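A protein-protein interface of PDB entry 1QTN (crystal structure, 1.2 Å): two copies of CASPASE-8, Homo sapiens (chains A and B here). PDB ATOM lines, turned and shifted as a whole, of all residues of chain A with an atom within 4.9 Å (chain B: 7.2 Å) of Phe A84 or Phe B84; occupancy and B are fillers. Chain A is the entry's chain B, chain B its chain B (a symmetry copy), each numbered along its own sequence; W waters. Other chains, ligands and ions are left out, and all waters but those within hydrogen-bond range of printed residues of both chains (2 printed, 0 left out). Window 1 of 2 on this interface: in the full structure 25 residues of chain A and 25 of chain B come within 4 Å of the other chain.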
ATOM      1  N   PHE A  15     -23.382  -8.615  19.188  1.00  0.00           N
ATOM      2  CA  PHE A  15     -23.056  -9.895  18.696  1.00  0.00           C
ATOM      3  C   PHE A  15     -21.511 -10.089  18.596  1.00  0.00           C
ATOM      4  O   PHE A  15     -20.757  -9.204  18.263  1.00  0.00           O
ATOM      5  CB  PHE A  15     -23.615 -10.154  17.286  1.00  0.00           C
ATOM      6  CG  PHE A  15     -25.086 -10.497  17.245  1.00  0.00           C
ATOM      7  CD1 PHE A  15     -26.056  -9.504  17.332  1.00  0.00           C
ATOM      8  CD2 PHE A  15     -25.510 -11.799  17.035  1.00  0.00           C
ATOM      9  CE1 PHE A  15     -27.391  -9.815  17.249  1.00  0.00           C
ATOM     10  CE2 PHE A  15     -26.845 -12.118  16.964  1.00  0.00           C
ATOM     11  CZ  PHE A  15     -27.804 -11.114  17.051  1.00  0.00           C
ATOM     12  N   LEU A  16     -21.171 -11.355  18.842  1.00  0.00           N
ATOM     13  CA  LEU A  16     -19.808 -11.842  18.574  1.00  0.00           C
ATOM     14  C   LEU A  16     -19.969 -13.175  17.827  1.00  0.00           C
ATOM     15  O   LEU A  16     -20.651 -14.078  18.326  1.00  0.00           O
ATOM     16  CB  LEU A  16     -19.040 -12.016  19.853  1.00  0.00           C
ATOM     17  CG  LEU A  16     -17.692 -12.751  19.781  1.00  0.00           C
ATOM     18  CD1 LEU A  16     -16.729 -12.005  18.912  1.00  0.00           C
ATOM     19  CD2 LEU A  16     -17.136 -12.933  21.190  1.00  0.00           C
ATOM     20  N   LEU A  56     -12.167 -10.660  23.088  1.00  0.00           N
ATOM     21  CA  LEU A  56     -11.429 -10.325  21.863  1.00  0.00           C
ATOM     22  C   LEU A  56      -9.968 -10.590  22.020  1.00  0.00           C
ATOM     23  O   LEU A  56      -9.275 -11.071  21.092  1.00  0.00           O
ATOM     24  CB  LEU A  56     -11.712  -8.881  21.450  1.00  0.00           C
ATOM     25  CG  LEU A  56     -13.157  -8.549  21.096  1.00  0.00           C
ATOM     26  CD1 LEU A  56     -13.251  -7.106  20.619  1.00  0.00           C
ATOM     27  CD2 LEU A  56     -13.718  -9.489  20.046  1.00  0.00           C
ATOM     28  N   LEU A  59      -9.725 -14.371  21.779  1.00  0.00           N
ATOM     29  CA  LEU A  59      -9.867 -14.810  20.414  1.00  0.00           C
ATOM     30  C   LEU A  59      -8.670 -14.495  19.550  1.00  0.00           C
ATOM     31  O   LEU A  59      -8.395 -15.224  18.582  1.00  0.00           O
ATOM     32  CB  LEU A  59     -11.175 -14.372  19.783  1.00  0.00           C
ATOM     33  CG  LEU A  59     -12.442 -15.051  20.312  1.00  0.00           C
ATOM     34  CD1 LEU A  59     -13.673 -14.303  19.839  1.00  0.00           C
ATOM     35  CD2 LEU A  59     -12.530 -16.511  19.875  1.00  0.00           C
ATOM     36  N   THR A  60      -7.953 -13.427  19.885  1.00  0.00           N
ATOM     37  CA  THR A  60      -6.677 -13.124  19.236  1.00  0.00           C
ATOM     38  C   THR A  60      -5.663 -14.237  19.529  1.00  0.00           C
ATOM     39  O   THR A  60      -4.941 -14.682  18.634  1.00  0.00           O
ATOM     40  CB  THR A  60      -6.153 -11.748  19.713  1.00  0.00           C
ATOM     41  OG1 THR A  60      -7.093 -10.737  19.225  1.00  0.00           O
ATOM     42  CG2 THR A  60      -4.833 -11.404  19.034  1.00  0.00           C
ATOM     43  N   ASN A  63      -6.481 -17.192  17.470  1.00  0.00           N
ATOM     44  CA  ASN A  63      -5.899 -16.972  16.138  1.00  0.00           C
ATOM     45  C   ASN A  63      -4.440 -17.334  16.102  1.00  0.00           C
ATOM     46  O   ASN A  63      -3.981 -17.996  15.145  1.00  0.00           O
ATOM     47  CB  ASN A  63      -6.155 -15.557  15.650  1.00  0.00           C
ATOM     48  CG  ASN A  63      -7.549 -15.243  15.212  1.00  0.00           C
ATOM     49  OD1 ASN A  63      -7.837 -14.002  14.965  1.00  0.00           O
ATOM     50  ND2 ASN A  63      -8.431 -16.163  15.080  1.00  0.00           N
ATOM     51  N   PRO A  80      -8.741 -18.956  11.842  1.00  0.00           N
ATOM     52  CA  PRO A  80     -10.038 -18.558  12.426  1.00  0.00           C
ATOM     53  C   PRO A  80     -10.277 -17.070  12.192  1.00  0.00           C
ATOM     54  O   PRO A  80      -9.366 -16.301  11.909  1.00  0.00           O
ATOM     55  CB  PRO A  80      -9.940 -18.949  13.870  1.00  0.00           C
ATOM     56  CG  PRO A  80      -8.840 -19.992  13.927  1.00  0.00           C
ATOM     57  CD  PRO A  80      -7.844 -19.479  12.876  1.00  0.00           C
ATOM     58  N   GLN A  81     -11.534 -16.665  12.470  1.00  0.00           N
ATOM     59  CA  GLN A  81     -11.912 -15.275  12.180  1.00  0.00           C
ATOM     60  C   GLN A  81     -13.116 -14.846  12.984  1.00  0.00           C
ATOM     61  O   GLN A  81     -14.271 -15.206  12.665  1.00  0.00           O
ATOM     62  CB  GLN A  81     -12.241 -15.228  10.682  1.00  0.00           C
ATOM     63  CG  GLN A  81     -12.671 -13.817  10.220  1.00  0.00           C
ATOM     64  CD  GLN A  81     -13.510 -13.984   8.948  1.00  0.00           C
ATOM     65  OE1 GLN A  81     -14.707 -14.325   9.097  1.00  0.00           O
ATOM     66  NE2 GLN A  81     -12.882 -14.035   7.834  1.00  0.00           N
ATOM     67  N   PRO A  82     -12.915 -13.978  13.962  1.00  0.00           N
ATOM     68  CA  PRO A  82     -14.086 -13.394  14.660  1.00  0.00           C
ATOM     69  C   PRO A  82     -14.604 -12.155  13.896  1.00  0.00           C
ATOM     70  O   PRO A  82     -13.853 -11.469  13.223  1.00  0.00           O
ATOM     71  CB  PRO A  82     -13.509 -12.920  16.008  1.00  0.00           C
ATOM     72  CG  PRO A  82     -12.235 -13.668  16.137  1.00  0.00           C
ATOM     73  CD  PRO A  82     -11.692 -13.777  14.747  1.00  0.00           C
ATOM     74  N   THR A  83     -15.883 -11.937  14.090  1.00  0.00           N
ATOM     75  CA  THR A  83     -16.587 -10.739  13.625  1.00  0.00           C
ATOM     76  C   THR A  83     -17.475 -10.247  14.763  1.00  0.00           C
ATOM     77  O   THR A  83     -17.992 -11.052  15.513  1.00  0.00           O
ATOM     78  CB  THR A  83     -17.496 -11.078  12.448  1.00  0.00           C
ATOM     79  OG1 THR A  83     -16.805 -11.545  11.349  1.00  0.00           O
ATOM     80  CG2 THR A  83     -18.218  -9.808  11.987  1.00  0.00           C
ATOM     81  N   PHE A  84     -17.612  -8.927  14.947  1.00  0.00           N
ATOM     82  CA  PHE A  84     -18.339  -8.472  16.128  1.00  0.00           C
ATOM     83  C   PHE A  84     -19.021  -7.123  15.931  1.00  0.00           C
ATOM     84  O   PHE A  84     -18.536  -6.234  15.209  1.00  0.00           O
ATOM     85  CB  PHE A  84     -17.437  -8.432  17.341  1.00  0.00           C
ATOM     86  CG  PHE A  84     -16.316  -7.439  17.343  1.00  0.00           C
ATOM     87  CD1 PHE A  84     -15.074  -7.737  16.794  1.00  0.00           C
ATOM     88  CD2 PHE A  84     -16.452  -6.181  17.946  1.00  0.00           C
ATOM     89  CE1 PHE A  84     -14.050  -6.840  16.826  1.00  0.00           C
ATOM     90  CE2 PHE A  84     -15.418  -5.290  18.005  1.00  0.00           C
ATOM     91  CZ  PHE A  84     -14.176  -5.627  17.447  1.00  0.00           C
ATOM     92  N   THR A  85     -20.128  -6.982  16.649  1.00  0.00           N
ATOM     93  CA  THR A  85     -20.837  -5.720  16.817  1.00  0.00           C
ATOM     94  C   THR A  85     -20.921  -5.363  18.291  1.00  0.00           C
ATOM     95  O   THR A  85     -21.723  -4.516  18.726  1.00  0.00           O
ATOM     96  CB  THR A  85     -22.199  -5.691  16.134  1.00  0.00           C
ATOM     97  OG1 THR A  85     -22.984  -6.728  16.692  1.00  0.00           O
ATOM     98  CG2 THR A  85     -22.106  -5.937  14.646  1.00  0.00           C
ATOM     99  N   LEU A  86     -20.061  -5.968  19.104  1.00  0.00           N
ATOM    100  CA  LEU A  86     -19.943  -5.653  20.518  1.00  0.00           C
ATOM    101  C   LEU A  86     -19.633  -4.160  20.706  1.00  0.00           C
ATOM    102  O   LEU A  86     -18.825  -3.597  19.956  1.00  0.00           O
ATOM    103  CB  LEU A  86     -18.814  -6.453  21.174  1.00  0.00           C
ATOM    104  CG  LEU A  86     -18.947  -7.972  21.153  1.00  0.00           C
ATOM    105  CD1 LEU A  86     -17.723  -8.558  21.866  1.00  0.00           C
ATOM    106  CD2 LEU A  86     -20.229  -8.432  21.831  1.00  0.00           C
ATOM    107  N   GLU B  12      -3.893 -15.853   5.031  1.00  0.00           N
ATOM    108  CA  GLU B  12      -4.893 -14.857   5.339  1.00  0.00           C
ATOM    109  C   GLU B  12      -4.772 -14.349   6.749  1.00  0.00           C
ATOM    110  O   GLU B  12      -5.705 -13.690   7.249  1.00  0.00           O
ATOM    111  CB  GLU B  12      -6.290 -15.297   4.963  1.00  0.00           C
ATOM    112  CG  GLU B  12      -6.506 -15.455   3.472  1.00  0.00           C
ATOM    113  CD  GLU B  12      -7.867 -15.952   3.083  1.00  0.00           C
ATOM    114  OE1 GLU B  12      -8.898 -15.445   3.571  1.00  0.00           O
ATOM    115  OE2 GLU B  12      -7.911 -16.988   2.349  1.00  0.00           O
ATOM    116  N   ASP B  14      -3.418 -11.959   9.929  1.00  0.00           N
ATOM    117  CA  ASP B  14      -3.003 -10.603  10.177  1.00  0.00           C
ATOM    118  C   ASP B  14      -3.776  -9.534   9.494  1.00  0.00           C
ATOM    119  O   ASP B  14      -3.255  -8.432   9.246  1.00  0.00           O
ATOM    120  CB  ASP B  14      -1.488 -10.418   9.995  1.00  0.00           C
ATOM    121  CG  ASP B  14      -0.684 -11.520  10.676  1.00  0.00           C
ATOM    122  OD1 ASP B  14      -0.890 -11.769  11.875  1.00  0.00           O
ATOM    123  OD2 ASP B  14       0.157 -12.161   9.988  1.00  0.00           O
ATOM    124  N   PHE B  15      -5.021  -9.703   9.149  1.00  0.00           N
ATOM    125  CA  PHE B  15      -5.932  -8.773   8.609  1.00  0.00           C
ATOM    126  C   PHE B  15      -6.916  -8.244   9.698  1.00  0.00           C
ATOM    127  O   PHE B  15      -7.359  -8.943  10.580  1.00  0.00           O
ATOM    128  CB  PHE B  15      -6.804  -9.371   7.492  1.00  0.00           C
ATOM    129  CG  PHE B  15      -6.117  -9.495   6.153  1.00  0.00           C
ATOM    130  CD1 PHE B  15      -5.246 -10.548   5.890  1.00  0.00           C
ATOM    131  CD2 PHE B  15      -6.397  -8.614   5.121  1.00  0.00           C
ATOM    132  CE1 PHE B  15      -4.658 -10.683   4.657  1.00  0.00           C
ATOM    133  CE2 PHE B  15      -5.800  -8.736   3.888  1.00  0.00           C
ATOM    134  CZ  PHE B  15      -4.933  -9.797   3.640  1.00  0.00           C
ATOM    135  N   LEU B  16      -7.249  -6.973   9.465  1.00  0.00           N
ATOM    136  CA  LEU B  16      -8.344  -6.326  10.206  1.00  0.00           C
ATOM    137  C   LEU B  16      -9.201  -5.602   9.157  1.00  0.00           C
ATOM    138  O   LEU B  16      -8.672  -4.790   8.388  1.00  0.00           O
ATOM    139  CB  LEU B  16      -7.805  -5.371  11.231  1.00  0.00           C
ATOM    140  CG  LEU B  16      -8.804  -4.427  11.921  1.00  0.00           C
ATOM    141  CD1 LEU B  16      -9.822  -5.206  12.692  1.00  0.00           C
ATOM    142  CD2 LEU B  16      -8.047  -3.460  12.826  1.00  0.00           C
ATOM    143  N   LEU B  17     -10.480  -5.926   9.127  1.00  0.00           N
ATOM    144  CA  LEU B  17     -11.423  -5.258   8.205  1.00  0.00           C
ATOM    145  C   LEU B  17     -12.465  -4.525   9.067  1.00  0.00           C
ATOM    146  O   LEU B  17     -13.216  -5.139   9.811  1.00  0.00           O
ATOM    147  CB  LEU B  17     -12.130  -6.309   7.365  1.00  0.00           C
ATOM    148  CG  LEU B  17     -13.289  -5.804   6.476  1.00  0.00           C
ATOM    149  CD1 LEU B  17     -12.755  -4.820   5.450  1.00  0.00           C
ATOM    150  CD2 LEU B  17     -13.964  -7.001   5.814  1.00  0.00           C
ATOM    151  N   VAL B  22     -22.887  -3.451   9.154  1.00  0.00           N
ATOM    152  CA  VAL B  22     -23.288  -4.809   8.906  1.00  0.00           C
ATOM    153  C   VAL B  22     -23.897  -4.916   7.501  1.00  0.00           C
ATOM    154  O   VAL B  22     -24.342  -3.937   6.900  1.00  0.00           O
ATOM    155  CB  VAL B  22     -24.338  -5.295   9.937  1.00  0.00           C
ATOM    156  CG1 VAL B  22     -23.761  -5.407  11.314  1.00  0.00           C
ATOM    157  CG2 VAL B  22     -25.600  -4.465   9.866  1.00  0.00           C
ATOM    158  N   ILE B  55      -6.310  -1.605  18.798  1.00  0.00           N
ATOM    159  CA  ILE B  55      -7.315  -1.282  17.793  1.00  0.00           C
ATOM    160  C   ILE B  55      -8.649  -1.943  18.026  1.00  0.00           C
ATOM    161  O   ILE B  55      -9.676  -1.366  17.634  1.00  0.00           O
ATOM    162  CB  ILE B  55      -6.821  -1.582  16.373  1.00  0.00           C
ATOM    163  CG1 ILE B  55      -7.622  -0.880  15.282  1.00  0.00           C
ATOM    164  CG2 ILE B  55      -6.920  -3.138  16.148  1.00  0.00           C
ATOM    165  CD1 ILE B  55      -7.682   0.615  15.388  1.00  0.00           C
ATOM    166  N   LEU B  56      -8.686  -3.144  18.567  1.00  0.00           N
ATOM    167  CA  LEU B  56      -9.972  -3.806  18.827  1.00  0.00           C
ATOM    168  C   LEU B  56     -10.726  -3.119  19.917  1.00  0.00           C
ATOM    169  O   LEU B  56     -11.970  -2.967  19.873  1.00  0.00           O
ATOM    170  CB  LEU B  56      -9.754  -5.289  19.124  1.00  0.00           C
ATOM    171  CG  LEU B  56      -9.147  -6.123  18.000  1.00  0.00           C
ATOM    172  CD1 LEU B  56      -9.085  -7.585  18.419  1.00  0.00           C
ATOM    173  CD2 LEU B  56      -9.917  -5.979  16.701  1.00  0.00           C
ATOM    174  N   THR B  57     -10.027  -2.614  20.917  1.00  0.00           N
ATOM    175  CA  THR B  57     -10.659  -1.800  21.961  1.00  0.00           C
ATOM    176  C   THR B  57     -11.181  -0.504  21.379  1.00  0.00           C
ATOM    177  O   THR B  57     -12.339  -0.094  21.632  1.00  0.00           O
ATOM    178  CB  THR B  57      -9.562  -1.489  23.036  1.00  0.00           C
ATOM    179  OG1 THR B  57      -9.221  -2.769  23.621  1.00  0.00           O
ATOM    180  CG2 THR B  57     -10.134  -0.625  24.121  1.00  0.00           C
ATOM    181  N   LEU B  59     -12.062   0.009  18.229  1.00  0.00           N
ATOM    182  CA  LEU B  59     -13.178  -0.305  17.374  1.00  0.00           C
ATOM    183  C   LEU B  59     -14.438  -0.657  18.128  1.00  0.00           C
ATOM    184  O   LEU B  59     -15.548  -0.428  17.622  1.00  0.00           O
ATOM    185  CB  LEU B  59     -12.836  -1.320  16.301  1.00  0.00           C
ATOM    186  CG  LEU B  59     -11.900  -0.839  15.188  1.00  0.00           C
ATOM    187  CD1 LEU B  59     -11.394  -2.020  14.383  1.00  0.00           C
ATOM    188  CD2 LEU B  59     -12.588   0.157  14.258  1.00  0.00           C
ATOM    189  N   THR B  60     -14.283  -1.204  19.331  1.00  0.00           N
ATOM    190  CA  THR B  60     -15.420  -1.424  20.226  1.00  0.00           C
ATOM    191  C   THR B  60     -16.047  -0.079  20.616  1.00  0.00           C
ATOM    192  O   THR B  60     -17.270   0.066  20.624  1.00  0.00           O
ATOM    193  CB  THR B  60     -14.965  -2.214  21.476  1.00  0.00           C
ATOM    194  OG1 THR B  60     -14.559  -3.545  21.020  1.00  0.00           O
ATOM    195  CG2 THR B  60     -16.137  -2.470  22.415  1.00  0.00           C
ATOM    196  N   GLU B  61     -15.222   0.899  20.936  1.00  0.00           N
ATOM    197  CA  GLU B  61     -15.703   2.245  21.235  1.00  0.00           C
ATOM    198  C   GLU B  61     -16.387   2.857  20.034  1.00  0.00           C
ATOM    199  O   GLU B  61     -17.443   3.506  20.206  1.00  0.00           O
ATOM    200  CB  GLU B  61     -14.577   3.135  21.734  1.00  0.00           C
ATOM    201  CG  GLU B  61     -14.961   4.601  21.881  1.00  0.00           C
ATOM    202  CD  GLU B  61     -13.959   5.418  22.653  1.00  0.00           C
ATOM    203  OE1 GLU B  61     -14.025   5.423  23.906  1.00  0.00           O
ATOM    204  OE2 GLU B  61     -13.124   6.105  22.020  1.00  0.00           O
ATOM    205  N   ASN B  63     -18.010   1.212  17.768  1.00  0.00           N
ATOM    206  CA  ASN B  63     -19.325   0.555  17.808  1.00  0.00           C
ATOM    207  C   ASN B  63     -20.256   1.232  18.774  1.00  0.00           C
ATOM    208  O   ASN B  63     -21.442   1.459  18.448  1.00  0.00           O
ATOM    209  CB  ASN B  63     -19.190  -0.932  18.082  1.00  0.00           C
ATOM    210  CG  ASN B  63     -18.681  -1.776  16.958  1.00  0.00           C
ATOM    211  OD1 ASN B  63     -18.385  -3.013  17.219  1.00  0.00           O
ATOM    212  ND2 ASN B  63     -18.545  -1.301  15.775  1.00  0.00           N
ATOM    213  N   MET B  79     -24.884   0.157  12.511  1.00  0.00           N
ATOM    214  CA  MET B  79     -24.082  -0.776  13.314  1.00  0.00           C
ATOM    215  C   MET B  79     -22.798  -1.161  12.575  1.00  0.00           C
ATOM    216  O   MET B  79     -22.828  -1.992  11.682  1.00  0.00           O
ATOM    217  CB  MET B  79     -24.897  -2.055  13.568  1.00  0.00           C
ATOM    218  CG  MET B  79     -24.196  -2.997  14.571  1.00  0.00           C
ATOM    219  SD  MET B  79     -24.129  -2.320  16.224  1.00  0.00           S
ATOM    220  CE  MET B  79     -22.415  -1.942  16.475  1.00  0.00           C
ATOM    221  N   PRO B  80     -21.676  -0.567  12.942  1.00  0.00           N
ATOM    222  CA  PRO B  80     -20.392  -0.973  12.334  1.00  0.00           C
ATOM    223  C   PRO B  80     -20.047  -2.397  12.756  1.00  0.00           C
ATOM    224  O   PRO B  80     -20.567  -2.933  13.727  1.00  0.00           O
ATOM    225  CB  PRO B  80     -19.411   0.064  12.794  1.00  0.00           C
ATOM    226  CG  PRO B  80     -20.253   1.261  13.192  1.00  0.00           C
ATOM    227  CD  PRO B  80     -21.496   0.600  13.809  1.00  0.00           C
ATOM    228  N   GLN B  81     -19.024  -2.943  12.065  1.00  0.00           N
ATOM    229  CA  GLN B  81     -18.673  -4.348  12.308  1.00  0.00           C
ATOM    230  C   GLN B  81     -17.257  -4.651  11.876  1.00  0.00           C
ATOM    231  O   GLN B  81     -16.968  -4.809  10.669  1.00  0.00           O
ATOM    232  CB  GLN B  81     -19.661  -5.182  11.483  1.00  0.00           C
ATOM    233  CG  GLN B  81     -19.411  -6.701  11.628  1.00  0.00           C
ATOM    234  CD  GLN B  81     -19.995  -7.385  10.387  1.00  0.00           C
ATOM    235  OE1 GLN B  81     -19.307  -7.349   9.341  1.00  0.00           O
ATOM    236  NE2 GLN B  81     -21.236  -7.700  10.422  1.00  0.00           N
ATOM    237  N   PRO B  82     -16.365  -4.865  12.828  1.00  0.00           N
ATOM    238  CA  PRO B  82     -15.010  -5.339  12.454  1.00  0.00           C
ATOM    239  C   PRO B  82     -14.996  -6.879  12.329  1.00  0.00           C
ATOM    240  O   PRO B  82     -15.758  -7.572  12.982  1.00  0.00           O
ATOM    241  CB  PRO B  82     -14.138  -4.947  13.662  1.00  0.00           C
ATOM    242  CG  PRO B  82     -14.940  -3.916  14.365  1.00  0.00           C
ATOM    243  CD  PRO B  82     -16.367  -4.336  14.196  1.00  0.00           C
ATOM    244  N   THR B  83     -14.077  -7.313  11.500  1.00  0.00           N
ATOM    245  CA  THR B  83     -13.735  -8.727  11.326  1.00  0.00           C
ATOM    246  C   THR B  83     -12.214  -8.840  11.305  1.00  0.00           C
ATOM    247  O   THR B  83     -11.552  -7.949  10.810  1.00  0.00           O
ATOM    248  CB  THR B  83     -14.253  -9.241   9.987  1.00  0.00           C
ATOM    249  OG1 THR B  83     -15.627  -9.183   9.880  1.00  0.00           O
ATOM    250  CG2 THR B  83     -13.878 -10.719   9.835  1.00  0.00           C
ATOM    251  N   PHE B  84     -11.641  -9.900  11.891  1.00  0.00           N
ATOM    252  CA  PHE B  84     -10.185  -9.918  11.996  1.00  0.00           C
ATOM    253  C   PHE B  84      -9.602 -11.327  12.017  1.00  0.00           C
ATOM    254  O   PHE B  84     -10.202 -12.285  12.536  1.00  0.00           O
ATOM    255  CB  PHE B  84      -9.715  -9.138  13.203  1.00  0.00           C
ATOM    256  CG  PHE B  84     -10.066  -9.671  14.557  1.00  0.00           C
ATOM    257  CD1 PHE B  84     -11.267  -9.348  15.182  1.00  0.00           C
ATOM    258  CD2 PHE B  84      -9.179 -10.479  15.280  1.00  0.00           C
ATOM    259  CE1 PHE B  84     -11.567  -9.812  16.426  1.00  0.00           C
ATOM    260  CE2 PHE B  84      -9.465 -10.924  16.542  1.00  0.00           C
ATOM    261  CZ  PHE B  84     -10.682 -10.572  17.143  1.00  0.00           C
ATOM    262  N   THR B  85      -8.386 -11.403  11.492  1.00  0.00           N
ATOM    263  CA  THR B  85      -7.523 -12.573  11.593  1.00  0.00           C
ATOM    264  C   THR B  85      -6.218 -12.200  12.274  1.00  0.00           C
ATOM    265  O   THR B  85      -5.205 -12.921  12.212  1.00  0.00           O
ATOM    266  CB  THR B  85      -7.303 -13.285  10.264  1.00  0.00           C
ATOM    267  OG1 THR B  85      -6.705 -12.360   9.374  1.00  0.00           O
ATOM    268  CG2 THR B  85      -8.595 -13.755   9.637  1.00  0.00           C
ATOM    269  N   LEU B  86      -6.214 -11.078  12.986  1.00  0.00           N
ATOM    270  CA  LEU B  86      -5.078 -10.643  13.784  1.00  0.00           C
ATOM    271  C   LEU B  86      -4.702 -11.726  14.807  1.00  0.00           C
ATOM    272  O   LEU B  86      -5.590 -12.336  15.416  1.00  0.00           O
ATOM    273  CB  LEU B  86      -5.399  -9.359  14.555  1.00  0.00           C
ATOM    274  CG  LEU B  86      -5.748  -8.129  13.724  1.00  0.00           C
ATOM    275  CD1 LEU B  86      -6.019  -6.974  14.694  1.00  0.00           C
ATOM    276  CD2 LEU B  86      -4.627  -7.766  12.762  1.00  0.00           C
ATOM    277  N   ARG B  87      -3.422 -11.918  15.000  1.00  0.00           N
ATOM    278  CA  ARG B  87      -2.847 -12.925  15.883  1.00  0.00           C
ATOM    279  C   ARG B  87      -2.121 -12.295  17.066  1.00  0.00           C
ATOM    280  O   ARG B  87      -1.695 -13.041  17.959  1.00  0.00           O
ATOM    281  CB  ARG B  87      -1.854 -13.802  15.130  1.00  0.00           C
ATOM    282  CG  ARG B  87      -2.365 -14.603  13.992  1.00  0.00           C
ATOM    283  CD  ARG B  87      -1.271 -15.302  13.193  1.00  0.00           C
ATOM    284  NE  ARG B  87      -0.255 -14.379  12.783  1.00  0.00           N
ATOM    285  CZ  ARG B  87       0.995 -14.261  13.197  1.00  0.00           C
ATOM    286  NH1 ARG B  87       1.568 -15.103  14.041  1.00  0.00           N
ATOM    287  NH2 ARG B  87       1.698 -13.235  12.776  1.00  0.00           N
ATOM    288  N   LYS B  88      -2.015 -10.987  17.100  1.00  0.00           N
ATOM    289  CA  LYS B  88      -1.393 -10.249  18.189  1.00  0.00           C
ATOM    290  C   LYS B  88      -2.217  -8.971  18.444  1.00  0.00           C
ATOM    291  O   LYS B  88      -3.052  -8.636  17.600  1.00  0.00           O
ATOM    292  CB  LYS B  88       0.044  -9.835  17.780  1.00  0.00           C
ATOM    293  CG  LYS B  88       0.926 -10.997  17.334  1.00  0.00           C
ATOM    294  CD  LYS B  88       2.328 -10.554  16.961  1.00  0.00           C
ATOM    295  CE  LYS B  88       3.215 -11.742  16.616  1.00  0.00           C
ATOM    296  NZ  LYS B  88       4.548 -11.281  16.096  1.00  0.00           N
HETATM  297  O   HOH W   1      -5.839  -8.199  18.227  1.00  0.00           O
HETATM  298  O   HOH W   2     -17.349 -11.042   8.615  1.00  0.00           O
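Among the printed residues, pairs that only touch across the chains: Thr A83 with Pro B82 (3.3 Å), Pro A82 with Thr B83 (3.3 Å), Gln A81 with Thr B83 (3.3 Å), Thr A83 with Gln B81 (3.3 Å), Thr A60 with Lys B88 (3.4 Å), Gln A81 with Phe B84 (3.5 Å), Phe A84 with Gln B81 (3.5 Å), Thr A60 with Arg B87 (3.5 Å), Thr A85 with Met B79 (3.5 Å), Thr A85 with Pro B80 (3.5 Å), Pro A80 with Thr B85 (3.5 Å), Thr A60 with Phe B84 (3.6 Å), Phe A84 with Thr B60 (3.6 Å), Thr A85 with Asn B63 (3.6 Å), Asn A63 with Thr B85 (3.6 Å), Thr A85 with Val B22 (3.8 Å), Phe A84 with Asn B63 (3.8 Å), Asn A63 with Phe B84 (3.8 Å), Thr A60 with Leu B86 (3.8 Å), Leu A86 with Thr B60 (3.8 Å), Leu A56 with Thr B60 (3.8 Å), Thr A60 with Leu B56 (3.8 Å), Phe A84 with Phe B84 (3.9 Å) and Asn A63 with Arg B87 (3.9 Å).
Water W2 lies within hydrogen-bond range of OG1 of Thr B83 (2.8 Å) and OG1 of Thr A83 (2.8 Å).
Water W1 lies within hydrogen-bond range of the backbone carbonyl oxygen of Lys B88 (2.9 Å) and the side-chain hydroxyl of Thr A60 (3.0 Å).
Of the printed residues of chain B, Thr A60 touches Leu B56, Phe B84, Leu B86, Arg B87 and Lys B88.
Printed residues of chain B within 4 Å of Thr A83: Gln B81 (3.3 Å), Pro B82 (3.3 Å) and Thr B83 (3.0 Å).
Leu B17 touches none of the printed residues of chain A.
Leu B59 touches none of the printed residues of chain A.
Of the printed residues of chain A, Asn B63 touches Phe A84 (3.8 Å), Thr A85 (3.6 Å) and Leu A86 (2.8 Å).
Phe B84 touches just these residues of chain A: Thr A60, Asn A63, Gln A81, Pro A82 and Phe A84.
Printed residues of chain A within 4 Å of Arg B87: Thr A60 (3.5 Å) and Asn A63 (3.9 Å).
The nearest residue of chain B that does not touch Phe A84 is Pro B80 (4.1 Å).
Printed residues of chain A that touch a printed residue of chain B: Leu A56, Thr A60, Asn A63, Pro A80, Gln A81, Pro A82, Thr A83, Phe A84, Thr A85 and Leu A86.
Of the 23 printed residues of chain B, 14 touch a printed residue of chain A.
Printed residues of chain B that touch a printed residue of chain A: Val B22, Leu B56, Thr B60, Asn B63, Met B79, Pro B80, Gln B81, Pro B82, Thr B83, Phe B84, Thr B85, Leu B86, Arg B87 and Lys B88.
Hydrophobic or aromatic side chains of chain B within 4 Å of the printed part of chain A: Val B22, Leu B56, Met B79, Pro B82 and Phe B84.
Among the printed residues, 29 pairs touch across the chains.
The backbone carbonyl oxygen (O) of Pro A80 is in hydrogen-bond range of the side-chain amide nitrogen (ND2) of Asn A63, 3.3 Å away.
The backbone carbonyl oxygen of Glu B12 lies within hydrogen-bond range of the side-chain hydroxyl of Thr B85, 2.7 Å away.
N of Leu B17 sits at hydrogen-bond distance from O of Thr B83 (2.8 Å).
O of Met B79 is in hydrogen-bond range of N of Val B22 (2.9 Å).
The side-chain amide nitrogen of Asn B63 sits at hydrogen-bond distance from the backbone carbonyl oxygen of Pro B80, 3.3 Å away.
Leu A56 touches Thr B60, and with the chains exchanged Thr A60 touches Leu B56.
Pro A80 touches Thr B85, and with the chains exchanged Thr A85 touches Pro B80.
Gln A81 touches Thr B83, and with the chains exchanged Thr A83 touches Gln B81.
Phe B84 touches its own counterpart, Phe A84.
Positions printed for both chains: 15, 16, 56, 59, 60, 63, 80, 81, 82, 83, 84, 85 and 86.
The side-chain amide oxygen (OD1) of Asn A63 sits close to the backbone carbonyl oxygen (O) of Leu B86 (2.8 Å).
The backbone carbonyl oxygen of Pro A82 is in hydrogen-bond range of the backbone NH of Phe B84.
The side-chain hydroxyl (OG1) of Thr A83 is in hydrogen-bond range of the side-chain hydroxyl (OG1) of Thr B83, 3.0 Å away.
The backbone NH (N) of Phe A84 sits at hydrogen-bond distance from the backbone carbonyl oxygen (O) of Pro B82, at 3.0 Å.
The backbone carbonyl oxygen (O) of Leu A86 lies close to the side-chain amide oxygen (OD1) of Asn B63 (2.8 Å).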
